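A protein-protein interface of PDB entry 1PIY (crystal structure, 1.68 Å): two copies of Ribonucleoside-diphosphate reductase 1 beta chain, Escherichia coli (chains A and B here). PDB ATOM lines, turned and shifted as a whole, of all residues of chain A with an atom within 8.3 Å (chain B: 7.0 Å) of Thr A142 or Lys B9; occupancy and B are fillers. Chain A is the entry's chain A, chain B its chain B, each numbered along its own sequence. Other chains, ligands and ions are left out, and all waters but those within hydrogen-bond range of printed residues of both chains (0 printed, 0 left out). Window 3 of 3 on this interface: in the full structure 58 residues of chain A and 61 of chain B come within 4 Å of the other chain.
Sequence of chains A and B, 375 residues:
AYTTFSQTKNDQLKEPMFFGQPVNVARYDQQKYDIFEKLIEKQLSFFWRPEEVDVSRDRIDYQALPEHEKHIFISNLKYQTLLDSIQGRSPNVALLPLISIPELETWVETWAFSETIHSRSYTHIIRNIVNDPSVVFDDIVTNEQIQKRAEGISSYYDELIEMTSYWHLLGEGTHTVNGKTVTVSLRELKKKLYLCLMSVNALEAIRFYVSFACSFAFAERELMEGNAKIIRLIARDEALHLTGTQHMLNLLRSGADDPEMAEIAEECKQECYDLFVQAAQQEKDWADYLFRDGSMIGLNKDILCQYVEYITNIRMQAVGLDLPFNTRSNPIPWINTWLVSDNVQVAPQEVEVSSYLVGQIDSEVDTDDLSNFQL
OE1 of Gln A147 lies close to O of Ile A140 (3.0 Å).
ND2 of Asn B24 is in hydrogen-bond range of O of Ser B6, 3.2 Å away.
The backbone carbonyl oxygen of Thr B8 lies close to the side-chain amide oxygen of Gln B21.
O of Thr B8 sits at hydrogen-bond distance from ND2 of Asn B24.
ND2 of Asn B24 lies close to ND2 of Asn B10, 3.4 Å away.
The side-chain amide nitrogen (ND2) of Asn B24 is in hydrogen-bond range of the side-chain amide oxygen (OE1) of Gln B21.
Among the printed residues, pairs that only touch across the chains: Thr A142 with Lys B9 (3.3 Å), Gln A147 with Phe B5 (3.4 Å), Val A141 with Gln B7 (3.6 Å), Asp A138 with Lys B9 (3.8 Å), Val A141 with Lys B9 (3.9 Å), Val A141 with Thr B8 (3.9 Å) and Val A141 with Asn B24 (3.9 Å).
Thr A142 touches one residue of chain B.
Of chain A, only Asp A138 (3.8 Å), Val A141 (3.9 Å) and Thr A142 (3.3 Å) come within 4 Å of Lys B9.
Printed residues of chain A within 4 Å of Thr B8: Val A141 (3.9 Å).
Of the printed residues of chain A, Gln B7 touches Val A141 (3.6 Å).
Of the printed residues of chain B, Asp A138 touches Lys B9.
Printed residues of chain B within 4 Å of Gln A147: Phe B5 (3.4 Å).
Of the 9 printed residues of chain B, 5 touch a printed residue of chain A.
Printed residues of chain B that touch a printed residue of chain A: Phe B5, Gln B7, Thr B8, Lys B9 and Asn B24.
Printed residues of chain A that touch a printed residue of chain B: Asp A138, Val A141, Thr A142 and Gln A147.
Hydrophobic or aromatic side chains of chain A within 4 Å of the printed part of chain B: Val A141.
Among the printed residues, 7 pairs touch across the chains.
Among the printed residues, no Asp or Glu carboxylate lies within 4 Å of a Lys or Arg side-chain nitrogen of the other chain.
No position is printed for both chains.
Of the 7 pairs that touch across the chains among the printed residues, none has its exchanged pair printed and touching as well.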
ATOM      1  N   LYS A  78     -23.401  11.733  11.827  1.00  0.00           N
ATOM      2  CA  LYS A  78     -23.580  11.107  13.138  1.00  0.00           C
ATOM      3  C   LYS A  78     -23.557  12.130  14.271  1.00  0.00           C
ATOM      4  O   LYS A  78     -24.324  12.024  15.234  1.00  0.00           O
ATOM      5  CB  LYS A  78     -22.515  10.030  13.369  1.00  0.00           C
ATOM      6  CG  LYS A  78     -22.740   8.789  12.503  1.00  0.00           C
ATOM      7  CD  LYS A  78     -21.806   7.633  12.845  1.00  0.00           C
ATOM      8  CE  LYS A  78     -20.403   7.831  12.301  1.00  0.00           C
ATOM      9  NZ  LYS A  78     -19.586   6.575  12.425  1.00  0.00           N
ATOM     10  N   SER A 134     -28.464   0.636  11.574  1.00  0.00           N
ATOM     11  CA  SER A 134     -28.056   0.259  12.921  1.00  0.00           C
ATOM     12  C   SER A 134     -26.564   0.450  13.159  1.00  0.00           C
ATOM     13  O   SER A 134     -26.146   0.787  14.265  1.00  0.00           O
ATOM     14  CB  SER A 134     -28.444  -1.193  13.206  1.00  0.00           C
ATOM     15  OG  SER A 134     -29.855  -1.343  13.194  1.00  0.00           O
ATOM     16  N   VAL A 135     -25.759   0.230  12.127  1.00  0.00           N
ATOM     17  CA  VAL A 135     -24.318   0.396  12.265  1.00  0.00           C
ATOM     18  C   VAL A 135     -24.007   1.860  12.548  1.00  0.00           C
ATOM     19  O   VAL A 135     -23.160   2.177  13.383  1.00  0.00           O
ATOM     20  CB  VAL A 135     -23.574  -0.034  10.981  1.00  0.00           C
ATOM     21  CG1 VAL A 135     -22.090   0.268  11.113  1.00  0.00           C
ATOM     22  CG2 VAL A 135     -23.785  -1.517  10.737  1.00  0.00           C
ATOM     23  N   VAL A 136     -24.709   2.746  11.851  1.00  0.00           N
ATOM     24  CA  VAL A 136     -24.517   4.182  12.012  1.00  0.00           C
ATOM     25  C   VAL A 136     -25.021   4.656  13.372  1.00  0.00           C
ATOM     26  O   VAL A 136     -24.286   5.294  14.125  1.00  0.00           O
ATOM     27  CB  VAL A 136     -25.254   4.966  10.899  1.00  0.00           C
ATOM     28  CG1 VAL A 136     -25.069   6.466  11.101  1.00  0.00           C
ATOM     29  CG2 VAL A 136     -24.724   4.548   9.540  1.00  0.00           C
ATOM     30  N   PHE A 137     -26.273   4.338  13.686  1.00  0.00           N
ATOM     31  CA  PHE A 137     -26.863   4.744  14.958  1.00  0.00           C
ATOM     32  C   PHE A 137     -26.127   4.180  16.170  1.00  0.00           C
ATOM     33  O   PHE A 137     -25.888   4.894  17.143  1.00  0.00           O
ATOM     34  CB  PHE A 137     -28.337   4.341  15.008  1.00  0.00           C
ATOM     35  CG  PHE A 137     -29.204   5.104  14.047  1.00  0.00           C
ATOM     36  CD1 PHE A 137     -29.279   6.493  14.113  1.00  0.00           C
ATOM     37  CD2 PHE A 137     -29.957   4.438  13.086  1.00  0.00           C
ATOM     38  CE1 PHE A 137     -30.091   7.211  13.235  1.00  0.00           C
ATOM     39  CE2 PHE A 137     -30.774   5.144  12.202  1.00  0.00           C
ATOM     40  CZ  PHE A 137     -30.840   6.537  12.279  1.00  0.00           C
ATOM     41  N   ASP A 138     -25.766   2.902  16.114  1.00  0.00           N
ATOM     42  CA  ASP A 138     -25.051   2.275  17.219  1.00  0.00           C
ATOM     43  C   ASP A 138     -23.705   2.950  17.465  1.00  0.00           C
ATOM     44  O   ASP A 138     -23.295   3.134  18.612  1.00  0.00           O
ATOM     45  CB  ASP A 138     -24.823   0.787  16.931  1.00  0.00           C
ATOM     46  CG  ASP A 138     -26.045  -0.063  17.227  1.00  0.00           C
ATOM     47  OD1 ASP A 138     -26.050  -1.250  16.836  1.00  0.00           O
ATOM     48  OD2 ASP A 138     -26.995   0.448  17.859  1.00  0.00           O
ATOM     49  N   ASP A 139     -23.023   3.325  16.389  1.00  0.00           N
ATOM     50  CA  ASP A 139     -21.717   3.956  16.517  1.00  0.00           C
ATOM     51  C   ASP A 139     -21.781   5.324  17.184  1.00  0.00           C
ATOM     52  O   ASP A 139     -20.832   5.744  17.849  1.00  0.00           O
ATOM     53  CB  ASP A 139     -21.051   4.075  15.146  1.00  0.00           C
ATOM     54  CG  ASP A 139     -19.594   4.452  15.249  1.00  0.00           C
ATOM     55  OD1 ASP A 139     -18.852   3.759  15.977  1.00  0.00           O
ATOM     56  OD2 ASP A 139     -19.189   5.438  14.605  1.00  0.00           O
ATOM     57  N   ILE A 140     -22.898   6.023  17.009  1.00  0.00           N
ATOM     58  CA  ILE A 140     -23.054   7.338  17.619  1.00  0.00           C
ATOM     59  C   ILE A 140     -22.833   7.235  19.125  1.00  0.00           C
ATOM     60  O   ILE A 140     -22.183   8.084  19.733  1.00  0.00           O
ATOM     61  CB  ILE A 140     -24.466   7.909  17.358  1.00  0.00           C
ATOM     62  CG1 ILE A 140     -24.644   8.185  15.863  1.00  0.00           C
ATOM     63  CG2 ILE A 140     -24.672   9.179  18.177  1.00  0.00           C
ATOM     64  CD1 ILE A 140     -26.046   8.617  15.477  1.00  0.00           C
ATOM     65  N   VAL A 141     -23.368   6.175  19.721  1.00  0.00           N
ATOM     66  CA  VAL A 141     -23.243   5.954  21.155  1.00  0.00           C
ATOM     67  C   VAL A 141     -21.844   5.507  21.582  1.00  0.00           C
ATOM     68  O   VAL A 141     -21.288   6.026  22.547  1.00  0.00           O
ATOM     69  CB  VAL A 141     -24.255   4.887  21.636  1.00  0.00           C
ATOM     70  CG1 VAL A 141     -24.143   4.698  23.142  1.00  0.00           C
ATOM     71  CG2 VAL A 141     -25.667   5.301  21.255  1.00  0.00           C
ATOM     72  N   THR A 142     -21.274   4.559  20.848  1.00  0.00           N
ATOM     73  CA  THR A 142     -19.963   4.016  21.195  1.00  0.00           C
ATOM     74  C   THR A 142     -18.729   4.729  20.649  1.00  0.00           C
ATOM     75  O   THR A 142     -17.621   4.483  21.122  1.00  0.00           O
ATOM     76  CB  THR A 142     -19.862   2.537  20.770  1.00  0.00           C
ATOM     77  OG1 THR A 142     -19.883   2.448  19.340  1.00  0.00           O
ATOM     78  CG2 THR A 142     -21.025   1.735  21.334  1.00  0.00           C
ATOM     79  N   ASN A 143     -18.902   5.600  19.661  1.00  0.00           N
ATOM     80  CA  ASN A 143     -17.760   6.293  19.069  1.00  0.00           C
ATOM     81  C   ASN A 143     -17.064   7.238  20.049  1.00  0.00           C
ATOM     82  O   ASN A 143     -17.584   8.306  20.370  1.00  0.00           O
ATOM     83  CB  ASN A 143     -18.210   7.067  17.829  1.00  0.00           C
ATOM     84  CG  ASN A 143     -17.049   7.507  16.966  1.00  0.00           C
ATOM     85  OD1 ASN A 143     -16.983   7.166  15.783  1.00  0.00           O
ATOM     86  ND2 ASN A 143     -16.128   8.265  17.545  1.00  0.00           N
ATOM     87  N   GLU A 144     -15.877   6.844  20.506  1.00  0.00           N
ATOM     88  CA  GLU A 144     -15.110   7.647  21.457  1.00  0.00           C
ATOM     89  C   GLU A 144     -14.857   9.078  20.985  1.00  0.00           C
ATOM     90  O   GLU A 144     -14.954  10.014  21.772  1.00  0.00           O
ATOM     91  CB  GLU A 144     -13.756   6.988  21.764  1.00  0.00           C
ATOM     92  CG  GLU A 144     -12.818   6.934  20.565  1.00  0.00           C
ATOM     93  CD  GLU A 144     -11.340   6.900  20.945  1.00  0.00           C
ATOM     94  OE1 GLU A 144     -10.498   6.932  20.019  1.00  0.00           O
ATOM     95  OE2 GLU A 144     -11.013   6.844  22.153  1.00  0.00           O
ATOM     96  N   GLN A 145     -14.523   9.246  19.709  1.00  0.00           N
ATOM     97  CA  GLN A 145     -14.245  10.575  19.176  1.00  0.00           C
ATOM     98  C   GLN A 145     -15.481  11.456  19.101  1.00  0.00           C
ATOM     99  O   GLN A 145     -15.399  12.669  19.294  1.00  0.00           O
ATOM    100  CB  GLN A 145     -13.592  10.471  17.798  1.00  0.00           C
ATOM    101  CG  GLN A 145     -12.176   9.936  17.859  1.00  0.00           C
ATOM    102  CD  GLN A 145     -11.333  10.681  18.885  1.00  0.00           C
ATOM    103  OE1 GLN A 145     -11.124  11.892  18.777  1.00  0.00           O
ATOM    104  NE2 GLN A 145     -10.851   9.959  19.890  1.00  0.00           N
ATOM    105  N   ILE A 146     -16.626  10.847  18.819  1.00  0.00           N
ATOM    106  CA  ILE A 146     -17.868  11.599  18.743  1.00  0.00           C
ATOM    107  C   ILE A 146     -18.268  12.060  20.140  1.00  0.00           C
ATOM    108  O   ILE A 146     -18.687  13.202  20.333  1.00  0.00           O
ATOM    109  CB  ILE A 146     -18.996  10.745  18.137  1.00  0.00           C
ATOM    110  CG1 ILE A 146     -18.691  10.469  16.662  1.00  0.00           C
ATOM    111  CG2 ILE A 146     -20.335  11.458  18.286  1.00  0.00           C
ATOM    112  CD1 ILE A 146     -19.715   9.589  15.974  1.00  0.00           C
ATOM    113  N   GLN A 147     -18.128  11.172  21.118  1.00  0.00           N
ATOM    114  CA  GLN A 147     -18.481  11.517  22.486  1.00  0.00           C
ATOM    115  C   GLN A 147     -17.470  12.478  23.105  1.00  0.00           C
ATOM    116  O   GLN A 147     -17.819  13.268  23.983  1.00  0.00           O
ATOM    117  CB  GLN A 147     -18.619  10.250  23.335  1.00  0.00           C
ATOM    118  CG  GLN A 147     -19.757   9.344  22.869  1.00  0.00           C
ATOM    119  CD  GLN A 147     -21.132   9.999  22.983  1.00  0.00           C
ATOM    120  OE1 GLN A 147     -22.081   9.601  22.303  1.00  0.00           O
ATOM    121  NE2 GLN A 147     -21.246  10.998  23.854  1.00  0.00           N
ATOM    122  N   LYS A 148     -16.220  12.422  22.654  1.00  0.00           N
ATOM    123  CA  LYS A 148     -15.206  13.333  23.179  1.00  0.00           C
ATOM    124  C   LYS A 148     -15.527  14.743  22.689  1.00  0.00           C
ATOM    125  O   LYS A 148     -15.353  15.724  23.414  1.00  0.00           O
ATOM    126  CB  LYS A 148     -13.806  12.923  22.705  1.00  0.00           C
ATOM    127  CG  LYS A 148     -13.297  11.647  23.351  1.00  0.00           C
ATOM    128  CD  LYS A 148     -13.132  11.815  24.856  1.00  0.00           C
ATOM    129  CE  LYS A 148     -13.158  10.474  25.581  1.00  0.00           C
ATOM    130  NZ  LYS A 148     -12.172   9.497  25.042  1.00  0.00           N
ATOM    131  N   PHE B   5     -28.535  11.555  27.806  1.00  0.00           N
ATOM    132  CA  PHE B   5     -27.933  10.698  26.788  1.00  0.00           C
ATOM    133  C   PHE B   5     -27.190   9.543  27.433  1.00  0.00           C
ATOM    134  O   PHE B   5     -26.008   9.650  27.756  1.00  0.00           O
ATOM    135  CB  PHE B   5     -26.971  11.459  25.871  1.00  0.00           C
ATOM    136  CG  PHE B   5     -26.637  10.706  24.607  1.00  0.00           C
ATOM    137  CD1 PHE B   5     -27.475  10.784  23.497  1.00  0.00           C
ATOM    138  CD2 PHE B   5     -25.529   9.869  24.551  1.00  0.00           C
ATOM    139  CE1 PHE B   5     -27.216  10.036  22.350  1.00  0.00           C
ATOM    140  CE2 PHE B   5     -25.260   9.117  23.410  1.00  0.00           C
ATOM    141  CZ  PHE B   5     -26.105   9.200  22.306  1.00  0.00           C
ATOM    142  N   SER B   6     -27.903   8.438  27.622  1.00  0.00           N
ATOM    143  CA  SER B   6     -27.318   7.251  28.220  1.00  0.00           C
ATOM    144  C   SER B   6     -26.161   6.788  27.343  1.00  0.00           C
ATOM    145  O   SER B   6     -26.306   6.626  26.131  1.00  0.00           O
ATOM    146  CB  SER B   6     -28.380   6.158  28.359  1.00  0.00           C
ATOM    147  OG  SER B   6     -29.130   6.013  27.165  1.00  0.00           O
ATOM    148  N   GLN B   7     -25.012   6.579  27.975  1.00  0.00           N
ATOM    149  CA  GLN B   7     -23.798   6.181  27.278  1.00  0.00           C
ATOM    150  C   GLN B   7     -23.667   4.693  26.987  1.00  0.00           C
ATOM    151  O   GLN B   7     -22.679   4.265  26.392  1.00  0.00           O
ATOM    152  CB  GLN B   7     -22.582   6.665  28.065  1.00  0.00           C
ATOM    153  N   THR B   8     -24.658   3.910  27.390  1.00  0.00           N
ATOM    154  CA  THR B   8     -24.628   2.472  27.154  1.00  0.00           C
ATOM    155  C   THR B   8     -25.312   2.136  25.842  1.00  0.00           C
ATOM    156  O   THR B   8     -26.417   2.602  25.573  1.00  0.00           O
ATOM    157  CB  THR B   8     -25.344   1.701  28.278  1.00  0.00           C
ATOM    158  OG1 THR B   8     -24.658   1.916  29.515  1.00  0.00           O
ATOM    159  CG2 THR B   8     -25.377   0.204  27.967  1.00  0.00           C
ATOM    160  N   LYS B   9     -24.651   1.335  25.016  1.00  0.00           N
ATOM    161  CA  LYS B   9     -25.253   0.939  23.755  1.00  0.00           C
ATOM    162  C   LYS B   9     -26.279  -0.119  24.132  1.00  0.00           C
ATOM    163  O   LYS B   9     -25.928  -1.154  24.702  1.00  0.00           O
ATOM    164  CB  LYS B   9     -24.203   0.352  22.806  1.00  0.00           C
ATOM    165  CG  LYS B   9     -24.702   0.177  21.375  1.00  0.00           C
ATOM    166  CD  LYS B   9     -23.562  -0.162  20.426  1.00  0.00           C
ATOM    167  CE  LYS B   9     -23.045  -1.575  20.632  1.00  0.00           C
ATOM    168  NZ  LYS B   9     -23.955  -2.585  20.009  1.00  0.00           N
ATOM    169  N   ASN B  10     -27.546   0.155  23.849  1.00  0.00           N
ATOM    170  CA  ASN B  10     -28.610  -0.786  24.175  1.00  0.00           C
ATOM    171  C   ASN B  10     -29.519  -1.058  22.986  1.00  0.00           C
ATOM    172  O   ASN B  10     -29.565  -0.281  22.029  1.00  0.00           O
ATOM    173  CB  ASN B  10     -29.455  -0.267  25.351  1.00  0.00           C
ATOM    174  CG  ASN B  10     -30.273   0.973  25.000  1.00  0.00           C
ATOM    175  OD1 ASN B  10     -31.391   1.147  25.493  1.00  0.00           O
ATOM    176  ND2 ASN B  10     -29.718   1.841  24.166  1.00  0.00           N
ATOM    177  N   ASP B  11     -30.234  -2.177  23.053  1.00  0.00           N
ATOM    178  CA  ASP B  11     -31.168  -2.551  22.001  1.00  0.00           C
ATOM    179  C   ASP B  11     -32.495  -1.896  22.353  1.00  0.00           C
ATOM    180  O   ASP B  11     -33.211  -2.364  23.235  1.00  0.00           O
ATOM    181  CB  ASP B  11     -31.351  -4.068  21.958  1.00  0.00           C
ATOM    182  CG  ASP B  11     -32.178  -4.515  20.773  1.00  0.00           C
ATOM    183  OD1 ASP B  11     -32.970  -3.698  20.259  1.00  0.00           O
ATOM    184  OD2 ASP B  11     -32.042  -5.688  20.359  1.00  0.00           O
ATOM    185  N   GLN B  21     -33.699   1.920  30.247  1.00  0.00           N
ATOM    186  CA  GLN B  21     -32.594   2.853  30.087  1.00  0.00           C
ATOM    187  C   GLN B  21     -33.111   4.076  29.325  1.00  0.00           C
ATOM    188  O   GLN B  21     -33.827   3.934  28.334  1.00  0.00           O
ATOM    189  CB  GLN B  21     -31.450   2.198  29.301  1.00  0.00           C
ATOM    190  CG  GLN B  21     -30.360   3.181  28.894  1.00  0.00           C
ATOM    191  CD  GLN B  21     -29.261   2.552  28.056  1.00  0.00           C
ATOM    192  OE1 GLN B  21     -28.609   3.236  27.265  1.00  0.00           O
ATOM    193  NE2 GLN B  21     -29.037   1.255  28.238  1.00  0.00           N
ATOM    194  N   ASN B  24     -31.218   7.203  24.244  1.00  0.00           N
ATOM    195  CA  ASN B  24     -30.059   7.973  23.842  1.00  0.00           C
ATOM    196  C   ASN B  24     -30.268   8.472  22.414  1.00  0.00           C
ATOM    197  O   ASN B  24     -30.633   9.625  22.218  1.00  0.00           O
ATOM    198  CB  ASN B  24     -28.733   7.184  23.981  1.00  0.00           C
ATOM    199  CG  ASN B  24     -28.823   5.733  23.518  1.00  0.00           C
ATOM    200  OD1 ASN B  24     -29.433   5.414  22.500  1.00  0.00           O
ATOM    201  ND2 ASN B  24     -28.172   4.847  24.264  1.00  0.00           N
